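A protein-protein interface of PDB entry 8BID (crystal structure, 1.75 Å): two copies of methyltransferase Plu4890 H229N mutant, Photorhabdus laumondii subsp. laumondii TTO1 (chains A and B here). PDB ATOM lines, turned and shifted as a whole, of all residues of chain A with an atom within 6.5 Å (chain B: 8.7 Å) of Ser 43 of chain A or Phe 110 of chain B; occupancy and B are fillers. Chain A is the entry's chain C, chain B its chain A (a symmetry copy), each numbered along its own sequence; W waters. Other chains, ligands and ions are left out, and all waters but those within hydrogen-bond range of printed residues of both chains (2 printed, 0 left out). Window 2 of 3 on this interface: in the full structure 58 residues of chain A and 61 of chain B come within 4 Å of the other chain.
The backbone carbonyl oxygen (O) of Leu 109 of chain B sits at hydrogen-bond distance from the backbone NH (N) of Asn 46 of chain A. The guanidinium group (NH1) of Arg 49 of chain A lies within hydrogen-bond range of the backbone carbonyl oxygen (O) of Ser 108 of chain B.
The backbone carbonyl oxygen (O) of Ala 18 of chain A sits at hydrogen-bond distance from the side-chain hydroxyl (OG1) of Thr 22 of chain A (2.7 Å). O of Leu 39 of chain A sits at hydrogen-bond distance from OG of Ser 43 of chain A (2.8 Å). O of Val 45 of chain A lies within hydrogen-bond range of OG of Ser 40 of chain A. The backbone NH of Val 45 of chain A lies close to the side-chain hydroxyl of Ser 43 of chain A (3.4 Å). N of Arg 49 of chain A sits at hydrogen-bond distance from OD1 of Asn 46 of chain A, at 2.9 Å. The backbone carbonyl oxygen of Tyr 105 of chain B lies within hydrogen-bond range of the side-chain hydroxyl of Ser 108 of chain B (2.6 Å).
CB of Ala 18 of chain A touches CD2 of Tyr 105 of chain B, at 3.4 Å. N of Gly 106 of chain B touches CB of Ala 18 of chain A, 3.8 Å away. Gly 106 of chain B touches Thr 22 of chain A. CZ of Phe 110 of chain B touches CD2 of Leu 24 of chain A (3.9 Å). Phe 110 of chain B touches Ser 43 of chain A (CE1 to O, 3.5 Å). Val 45 of chain A touches Leu 109 of chain B (CA to O, 3.5 Å). N of Val 45 of chain A touches CD1 of Phe 110 of chain B, at 3.98 Å. Arg 49 of chain A touches Leu 109 of chain B (NH2 to CD2, 3.6 Å).
Glu 38 of chain A touches none of the printed residues of chain B. Ser 43 of chain A touches just one residue of chain B: Phe 110 (3.5 Å). Of the printed residues of chain B, Arg 49 of chain A touches Ser 108 (2.9 Å) and Leu 109 (3.6 Å). Of the printed residues of chain A, Tyr 105 of chain B touches Ala 18 (3.4 Å). Of the printed residues of chain A, Phe 110 of chain B touches Leu 24 (3.9 Å), Ser 43 (3.5 Å) and Val 45 (3.98 Å). Lys 115 of chain B touches none of the printed residues of chain A. The nearest residue of chain B that does not touch Ser 43 of chain A is Leu 109 of chain B (7.2 Å). The nearest printed residue of chain A that does not touch Gly 106 of chain B is Leu 24 of chain A (5.6 Å).
Of the 14 printed residues of chain A, 7 touch a printed residue of chain B. Along chain A the printed residues that touch a printed residue of chain B span positions 18 to 49.
No position is printed for both chains.
Water W1 lies within hydrogen-bond range of OH of Tyr 105 of chain B (2.6 Å) and O of Arg 49 of chain A (2.7 Å). Water W2 bridges OG of Ser 108 of chain B (3.3 Å) and NH2 of Arg 49 of chain A (3.5 Å).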
ATOM      1  N   ALA A  18     -29.191  22.219 -39.974  1.00  0.00           N
ATOM      2  CA  ALA A  18     -28.842  21.939 -38.559  1.00  0.00           C
ATOM      3  C   ALA A  18     -30.089  22.072 -37.669  1.00  0.00           C
ATOM      4  O   ALA A  18     -30.257  21.237 -36.765  1.00  0.00           O
ATOM      5  CB  ALA A  18     -27.734  22.859 -38.109  1.00  0.00           C
ATOM      6  N   THR A  22     -31.997  17.958 -37.091  1.00  0.00           N
ATOM      7  CA  THR A  22     -31.808  17.546 -35.673  1.00  0.00           C
ATOM      8  C   THR A  22     -33.167  17.351 -34.984  1.00  0.00           C
ATOM      9  O   THR A  22     -33.185  16.801 -33.884  1.00  0.00           O
ATOM     10  CB  THR A  22     -30.991  18.575 -34.876  1.00  0.00           C
ATOM     11  OG1 THR A  22     -31.701  19.818 -34.920  1.00  0.00           O
ATOM     12  CG2 THR A  22     -29.572  18.734 -35.383  1.00  0.00           C
ATOM     13  N   LEU A  24     -34.792  19.928 -33.818  1.00  0.00           N
ATOM     14  CA  LEU A  24     -34.907  21.093 -32.889  1.00  0.00           C
ATOM     15  C   LEU A  24     -36.156  21.910 -33.258  1.00  0.00           C
ATOM     16  O   LEU A  24     -36.898  22.312 -32.327  1.00  0.00           O
ATOM     17  CB  LEU A  24     -33.637  21.953 -32.943  1.00  0.00           C
ATOM     18  CG  LEU A  24     -32.458  21.454 -32.108  1.00  0.00           C
ATOM     19  CD1 LEU A  24     -31.173  22.161 -32.497  1.00  0.00           C
ATOM     20  CD2 LEU A  24     -32.721  21.637 -30.624  1.00  0.00           C
ATOM     21  N   HIS A  27     -39.868  21.649 -31.910  1.00  0.00           N
ATOM     22  CA  HIS A  27     -40.219  22.240 -30.588  1.00  0.00           C
ATOM     23  C   HIS A  27     -40.965  23.564 -30.778  1.00  0.00           C
ATOM     24  O   HIS A  27     -41.342  24.162 -29.764  1.00  0.00           O
ATOM     25  CB  HIS A  27     -38.965  22.419 -29.719  1.00  0.00           C
ATOM     26  CG  HIS A  27     -38.399  21.132 -29.216  1.00  0.00           C
ATOM     27  ND1 HIS A  27     -38.765  20.598 -27.991  1.00  0.00           N
ATOM     28  CD2 HIS A  27     -37.501  20.277 -29.757  1.00  0.00           C
ATOM     29  CE1 HIS A  27     -38.119  19.463 -27.802  1.00  0.00           C
ATOM     30  NE2 HIS A  27     -37.334  19.246 -28.873  1.00  0.00           N
ATOM     31  N   GLU A  38     -34.774  26.970 -21.558  1.00  0.00           N
ATOM     32  CA  GLU A  38     -35.667  25.807 -21.273  1.00  0.00           C
ATOM     33  C   GLU A  38     -35.379  24.692 -22.290  1.00  0.00           C
ATOM     34  O   GLU A  38     -35.187  23.537 -21.865  1.00  0.00           O
ATOM     35  CB  GLU A  38     -37.143  26.208 -21.310  1.00  0.00           C
ATOM     36  CG  GLU A  38     -37.553  27.154 -20.193  1.00  0.00           C
ATOM     37  CD  GLU A  38     -38.967  27.705 -20.291  1.00  0.00           C
ATOM     38  OE1 GLU A  38     -39.712  27.276 -21.201  1.00  0.00           O
ATOM     39  OE2 GLU A  38     -39.325  28.571 -19.457  1.00  0.00           O
ATOM     40  N   LEU A  39     -35.335  25.023 -23.581  1.00  0.00           N
ATOM     41  CA  LEU A  39     -35.077  24.037 -24.667  1.00  0.00           C
ATOM     42  C   LEU A  39     -33.744  23.313 -24.422  1.00  0.00           C
ATOM     43  O   LEU A  39     -33.712  22.081 -24.610  1.00  0.00           O
ATOM     44  CB  LEU A  39     -35.080  24.745 -26.024  1.00  0.00           C
ATOM     45  CG  LEU A  39     -34.882  23.829 -27.232  1.00  0.00           C
ATOM     46  CD1 LEU A  39     -35.906  22.699 -27.241  1.00  0.00           C
ATOM     47  CD2 LEU A  39     -34.952  24.623 -28.528  1.00  0.00           C
ATOM     48  N   SER A  40     -32.692  24.043 -24.029  1.00  0.00           N
ATOM     49  CA  SER A  40     -31.341  23.501 -23.707  1.00  0.00           C
ATOM     50  C   SER A  40     -31.428  22.485 -22.559  1.00  0.00           C
ATOM     51  O   SER A  40     -30.892  21.369 -22.707  1.00  0.00           O
ATOM     52  CB  SER A  40     -30.371  24.613 -23.383  1.00  0.00           C
ATOM     53  OG  SER A  40     -29.150  24.088 -22.883  1.00  0.00           O
ATOM     54  N   ARG A  41     -32.076  22.872 -21.460  1.00  0.00           N
ATOM     55  CA  ARG A  41     -32.292  22.037 -20.246  1.00  0.00           C
ATOM     56  C   ARG A  41     -32.958  20.715 -20.649  1.00  0.00           C
ATOM     57  O   ARG A  41     -32.532  19.661 -20.155  1.00  0.00           O
ATOM     58  CB  ARG A  41     -33.173  22.803 -19.252  1.00  0.00           C
ATOM     59  CG  ARG A  41     -32.663  22.810 -17.819  1.00  0.00           C
ATOM     60  CD  ARG A  41     -33.549  23.654 -16.917  1.00  0.00           C
ATOM     61  NE  ARG A  41     -33.399  25.089 -17.167  1.00  0.00           N
ATOM     62  CZ  ARG A  41     -34.377  25.936 -17.505  1.00  0.00           C
ATOM     63  NH1 ARG A  41     -34.094  27.213 -17.708  1.00  0.00           N
ATOM     64  NH2 ARG A  41     -35.628  25.521 -17.631  1.00  0.00           N
ATOM     65  N   LYS A  42     -33.956  20.787 -21.533  1.00  0.00           N
ATOM     66  CA  LYS A  42     -34.834  19.657 -21.928  1.00  0.00           C
ATOM     67  C   LYS A  42     -34.112  18.730 -22.912  1.00  0.00           C
ATOM     68  O   LYS A  42     -34.166  17.511 -22.692  1.00  0.00           O
ATOM     69  CB  LYS A  42     -36.125  20.205 -22.543  1.00  0.00           C
ATOM     70  CG  LYS A  42     -37.118  19.164 -23.043  1.00  0.00           C
ATOM     71  CD  LYS A  42     -38.387  19.775 -23.599  1.00  0.00           C
ATOM     72  CE  LYS A  42     -39.440  18.743 -23.944  1.00  0.00           C
ATOM     73  NZ  LYS A  42     -40.683  19.379 -24.442  1.00  0.00           N
ATOM     74  N   SER A  43     -33.487  19.286 -23.961  1.00  0.00           N
ATOM     75  CA  SER A  43     -32.943  18.538 -25.130  1.00  0.00           C
ATOM     76  C   SER A  43     -31.427  18.309 -25.018  1.00  0.00           C
ATOM     77  O   SER A  43     -30.932  17.415 -25.728  1.00  0.00           O
ATOM     78  CB  SER A  43     -33.275  19.251 -26.419  1.00  0.00           C
ATOM     79  OG  SER A  43     -32.505  20.436 -26.544  1.00  0.00           O
ATOM     80  N   GLY A  44     -30.720  19.098 -24.199  1.00  0.00           N
ATOM     81  CA  GLY A  44     -29.259  19.020 -24.005  1.00  0.00           C
ATOM     82  C   GLY A  44     -28.495  19.769 -25.089  1.00  0.00           C
ATOM     83  O   GLY A  44     -27.258  19.608 -25.152  1.00  0.00           O
ATOM     84  N   VAL A  45     -29.184  20.572 -25.912  1.00  0.00           N
ATOM     85  CA  VAL A  45     -28.539  21.450 -26.935  1.00  0.00           C
ATOM     86  C   VAL A  45     -27.782  22.551 -26.184  1.00  0.00           C
ATOM     87  O   VAL A  45     -28.257  22.969 -25.107  1.00  0.00           O
ATOM     88  CB  VAL A  45     -29.548  22.030 -27.948  1.00  0.00           C
ATOM     89  CG1 VAL A  45     -30.495  23.048 -27.326  1.00  0.00           C
ATOM     90  CG2 VAL A  45     -28.841  22.637 -29.147  1.00  0.00           C
ATOM     91  N   ASN A  46     -26.625  22.965 -26.700  1.00  0.00           N
ATOM     92  CA  ASN A  46     -25.791  24.040 -26.097  1.00  0.00           C
ATOM     93  C   ASN A  46     -26.558  25.365 -26.193  1.00  0.00           C
ATOM     94  O   ASN A  46     -26.896  25.772 -27.326  1.00  0.00           O
ATOM     95  CB  ASN A  46     -24.419  24.146 -26.764  1.00  0.00           C
ATOM     96  CG  ASN A  46     -23.514  25.124 -26.048  1.00  0.00           C
ATOM     97  OD1 ASN A  46     -23.529  26.316 -26.340  1.00  0.00           O
ATOM     98  ND2 ASN A  46     -22.760  24.640 -25.080  1.00  0.00           N
ATOM     99  N   ARG A  49     -24.465  28.476 -28.008  1.00  0.00           N
ATOM    100  CA  ARG A  49     -24.165  28.168 -29.434  1.00  0.00           C
ATOM    101  C   ARG A  49     -25.482  28.059 -30.213  1.00  0.00           C
ATOM    102  O   ARG A  49     -25.529  28.527 -31.380  1.00  0.00           O
ATOM    103  CB  ARG A  49     -23.315  26.899 -29.539  1.00  0.00           C
ATOM    104  CG  ARG A  49     -21.914  27.047 -28.956  1.00  0.00           C
ATOM    105  CD  ARG A  49     -21.135  25.751 -29.023  1.00  0.00           C
ATOM    106  NE  ARG A  49     -21.185  25.216 -30.381  1.00  0.00           N
ATOM    107  CZ  ARG A  49     -21.348  23.934 -30.706  1.00  0.00           C
ATOM    108  NH1 ARG A  49     -21.461  22.998 -29.779  1.00  0.00           N
ATOM    109  NH2 ARG A  49     -21.406  23.589 -31.974  1.00  0.00           N
ATOM    110  N   MET B 104     -22.098  17.952 -39.826  1.00  0.00           N
ATOM    111  CA  MET B 104     -21.923  17.577 -38.398  1.00  0.00           C
ATOM    112  C   MET B 104     -22.347  18.724 -37.470  1.00  0.00           C
ATOM    113  O   MET B 104     -22.372  18.497 -36.236  1.00  0.00           O
ATOM    114  CB  MET B 104     -20.472  17.190 -38.104  1.00  0.00           C
ATOM    115  CG  MET B 104     -20.088  15.849 -38.687  1.00  0.00           C
ATOM    116  SD  MET B 104     -20.952  14.472 -37.900  1.00  0.00           S
ATOM    117  CE  MET B 104     -21.422  13.529 -39.348  1.00  0.00           C
ATOM    118  N   TYR B 105     -22.707  19.891 -38.017  1.00  0.00           N
ATOM    119  CA  TYR B 105     -23.022  21.107 -37.216  1.00  0.00           C
ATOM    120  C   TYR B 105     -24.152  20.796 -36.225  1.00  0.00           C
ATOM    121  O   TYR B 105     -23.985  21.055 -35.020  1.00  0.00           O
ATOM    122  CB  TYR B 105     -23.356  22.293 -38.121  1.00  0.00           C
ATOM    123  CG  TYR B 105     -23.746  23.565 -37.408  1.00  0.00           C
ATOM    124  CD1 TYR B 105     -23.135  23.960 -36.227  1.00  0.00           C
ATOM    125  CD2 TYR B 105     -24.716  24.397 -37.937  1.00  0.00           C
ATOM    126  CE1 TYR B 105     -23.506  25.126 -35.573  1.00  0.00           C
ATOM    127  CE2 TYR B 105     -25.093  25.569 -37.303  1.00  0.00           C
ATOM    128  CZ  TYR B 105     -24.490  25.935 -36.114  1.00  0.00           C
ATOM    129  OH  TYR B 105     -24.872  27.089 -35.496  1.00  0.00           O
ATOM    130  N   GLY B 106     -25.271  20.268 -36.723  1.00  0.00           N
ATOM    131  CA  GLY B 106     -26.445  19.915 -35.899  1.00  0.00           C
ATOM    132  C   GLY B 106     -26.057  19.049 -34.712  1.00  0.00           C
ATOM    133  O   GLY B 106     -26.403  19.412 -33.572  1.00  0.00           O
ATOM    134  N   LYS B 107     -25.349  17.946 -34.971  1.00  0.00           N
ATOM    135  CA  LYS B 107     -24.906  16.966 -33.945  1.00  0.00           C
ATOM    136  C   LYS B 107     -23.948  17.657 -32.969  1.00  0.00           C
ATOM    137  O   LYS B 107     -24.103  17.439 -31.752  1.00  0.00           O
ATOM    138  CB  LYS B 107     -24.244  15.747 -34.596  1.00  0.00           C
ATOM    139  CG  LYS B 107     -25.160  14.919 -35.485  1.00  0.00           C
ATOM    140  CD  LYS B 107     -24.419  13.992 -36.434  1.00  0.00           C
ATOM    141  CE  LYS B 107     -25.282  13.495 -37.573  1.00  0.00           C
ATOM    142  NZ  LYS B 107     -26.549  12.908 -37.077  1.00  0.00           N
ATOM    143  N   SER B 108     -23.022  18.478 -33.479  1.00  0.00           N
ATOM    144  CA  SER B 108     -22.016  19.223 -32.670  1.00  0.00           C
ATOM    145  C   SER B 108     -22.707  20.045 -31.577  1.00  0.00           C
ATOM    146  O   SER B 108     -22.064  20.288 -30.551  1.00  0.00           O
ATOM    147  CB  SER B 108     -21.133  20.116 -33.517  1.00  0.00           C
ATOM    148  OG  SER B 108     -21.762  21.368 -33.782  1.00  0.00           O
ATOM    149  N   LEU B 109     -23.952  20.481 -31.787  1.00  0.00           N
ATOM    150  CA  LEU B 109     -24.671  21.348 -30.812  1.00  0.00           C
ATOM    151  C   LEU B 109     -25.111  20.536 -29.590  1.00  0.00           C
ATOM    152  O   LEU B 109     -25.498  21.172 -28.603  1.00  0.00           O
ATOM    153  CB  LEU B 109     -25.883  22.003 -31.479  1.00  0.00           C
ATOM    154  CG  LEU B 109     -25.574  23.014 -32.583  1.00  0.00           C
ATOM    155  CD1 LEU B 109     -26.835  23.347 -33.357  1.00  0.00           C
ATOM    156  CD2 LEU B 109     -24.951  24.282 -32.016  1.00  0.00           C
ATOM    157  N   PHE B 110     -25.068  19.200 -29.654  1.00  0.00           N
ATOM    158  CA  PHE B 110     -25.513  18.298 -28.557  1.00  0.00           C
ATOM    159  C   PHE B 110     -24.312  17.697 -27.819  1.00  0.00           C
ATOM    160  O   PHE B 110     -24.533  17.009 -26.820  1.00  0.00           O
ATOM    161  CB  PHE B 110     -26.420  17.194 -29.107  1.00  0.00           C
ATOM    162  CG  PHE B 110     -27.778  17.673 -29.554  1.00  0.00           C
ATOM    163  CD1 PHE B 110     -28.841  17.712 -28.664  1.00  0.00           C
ATOM    164  CD2 PHE B 110     -27.989  18.090 -30.860  1.00  0.00           C
ATOM    165  CE1 PHE B 110     -30.093  18.151 -29.074  1.00  0.00           C
ATOM    166  CE2 PHE B 110     -29.239  18.533 -31.264  1.00  0.00           C
ATOM    167  CZ  PHE B 110     -30.289  18.564 -30.371  1.00  0.00           C
ATOM    168  N   GLU B 111     -23.087  17.947 -28.287  1.00  0.00           N
ATOM    169  CA  GLU B 111     -21.837  17.407 -27.683  1.00  0.00           C
ATOM    170  C   GLU B 111     -21.202  18.475 -26.784  1.00  0.00           C
ATOM    171  O   GLU B 111     -21.439  19.682 -27.015  1.00  0.00           O
ATOM    172  CB  GLU B 111     -20.869  16.945 -28.774  1.00  0.00           C
ATOM    173  CG  GLU B 111     -21.476  15.966 -29.771  1.00  0.00           C
ATOM    174  CD  GLU B 111     -22.065  14.693 -29.180  1.00  0.00           C
ATOM    175  OE1 GLU B 111     -22.945  14.092 -29.836  1.00  0.00           O
ATOM    176  OE2 GLU B 111     -21.648  14.305 -28.067  1.00  0.00           O
ATOM    177  N   ASP B 112     -20.427  18.032 -25.792  1.00  0.00           N
ATOM    178  CA  ASP B 112     -19.811  18.885 -24.740  1.00  0.00           C
ATOM    179  C   ASP B 112     -18.343  18.481 -24.555  1.00  0.00           C
ATOM    180  O   ASP B 112     -17.780  18.798 -23.492  1.00  0.00           O
ATOM    181  CB  ASP B 112     -20.613  18.767 -23.437  1.00  0.00           C
ATOM    182  CG  ASP B 112     -20.329  19.871 -22.434  1.00  0.00           C
ATOM    183  OD1 ASP B 112     -20.229  21.039 -22.862  1.00  0.00           O
ATOM    184  OD2 ASP B 112     -20.197  19.553 -21.238  1.00  0.00           O
ATOM    185  N   ASP B 113     -17.748  17.823 -25.560  1.00  0.00           N
ATOM    186  CA  ASP B 113     -16.358  17.286 -25.527  1.00  0.00           C
ATOM    187  C   ASP B 113     -15.394  18.285 -26.182  1.00  0.00           C
ATOM    188  O   ASP B 113     -14.224  17.921 -26.366  1.00  0.00           O
ATOM    189  CB  ASP B 113     -16.253  15.936 -26.244  1.00  0.00           C
ATOM    190  CG  ASP B 113     -17.185  14.853 -25.724  1.00  0.00           C
ATOM    191  OD1 ASP B 113     -17.600  14.942 -24.550  1.00  0.00           O
ATOM    192  OD2 ASP B 113     -17.485  13.922 -26.503  1.00  0.00           O
ATOM    193  N   LYS B 115     -15.265  19.347 -29.262  1.00  0.00           N
ATOM    194  CA  LYS B 115     -14.905  18.995 -30.662  1.00  0.00           C
ATOM    195  C   LYS B 115     -15.765  19.820 -31.623  1.00  0.00           C
ATOM    196  O   LYS B 115     -17.000  19.746 -31.542  1.00  0.00           O
ATOM    197  CB  LYS B 115     -15.036  17.489 -30.898  1.00  0.00           C
ATOM    198  CG  LYS B 115     -13.946  16.663 -30.231  1.00  0.00           C
ATOM    199  CD  LYS B 115     -13.993  15.197 -30.576  1.00  0.00           C
ATOM    200  CE  LYS B 115     -13.083  14.368 -29.697  1.00  0.00           C
ATOM    201  NZ  LYS B 115     -13.203  12.928 -30.013  1.00  0.00           N
ATOM    202  N   MET B 120     -15.291  16.516 -35.757  1.00  0.00           N
ATOM    203  CA  MET B 120     -16.225  15.360 -35.788  1.00  0.00           C
ATOM    204  C   MET B 120     -16.219  14.710 -37.181  1.00  0.00           C
ATOM    205  O   MET B 120     -16.272  13.475 -37.249  1.00  0.00           O
ATOM    206  CB  MET B 120     -17.640  15.794 -35.395  1.00  0.00           C
ATOM    207  CG  MET B 120     -17.749  16.149 -33.917  1.00  0.00           C
ATOM    208  SD  MET B 120     -19.324  16.930 -33.486  1.00  0.00           S
ATOM    209  CE  MET B 120     -20.448  15.562 -33.756  1.00  0.00           C
HETATM  210  O   HOH W   1     -23.770  28.050 -33.385  1.00  0.00           O
HETATM  211  O   HOH W   2     -18.966  23.033 -34.365  1.00  0.00           O
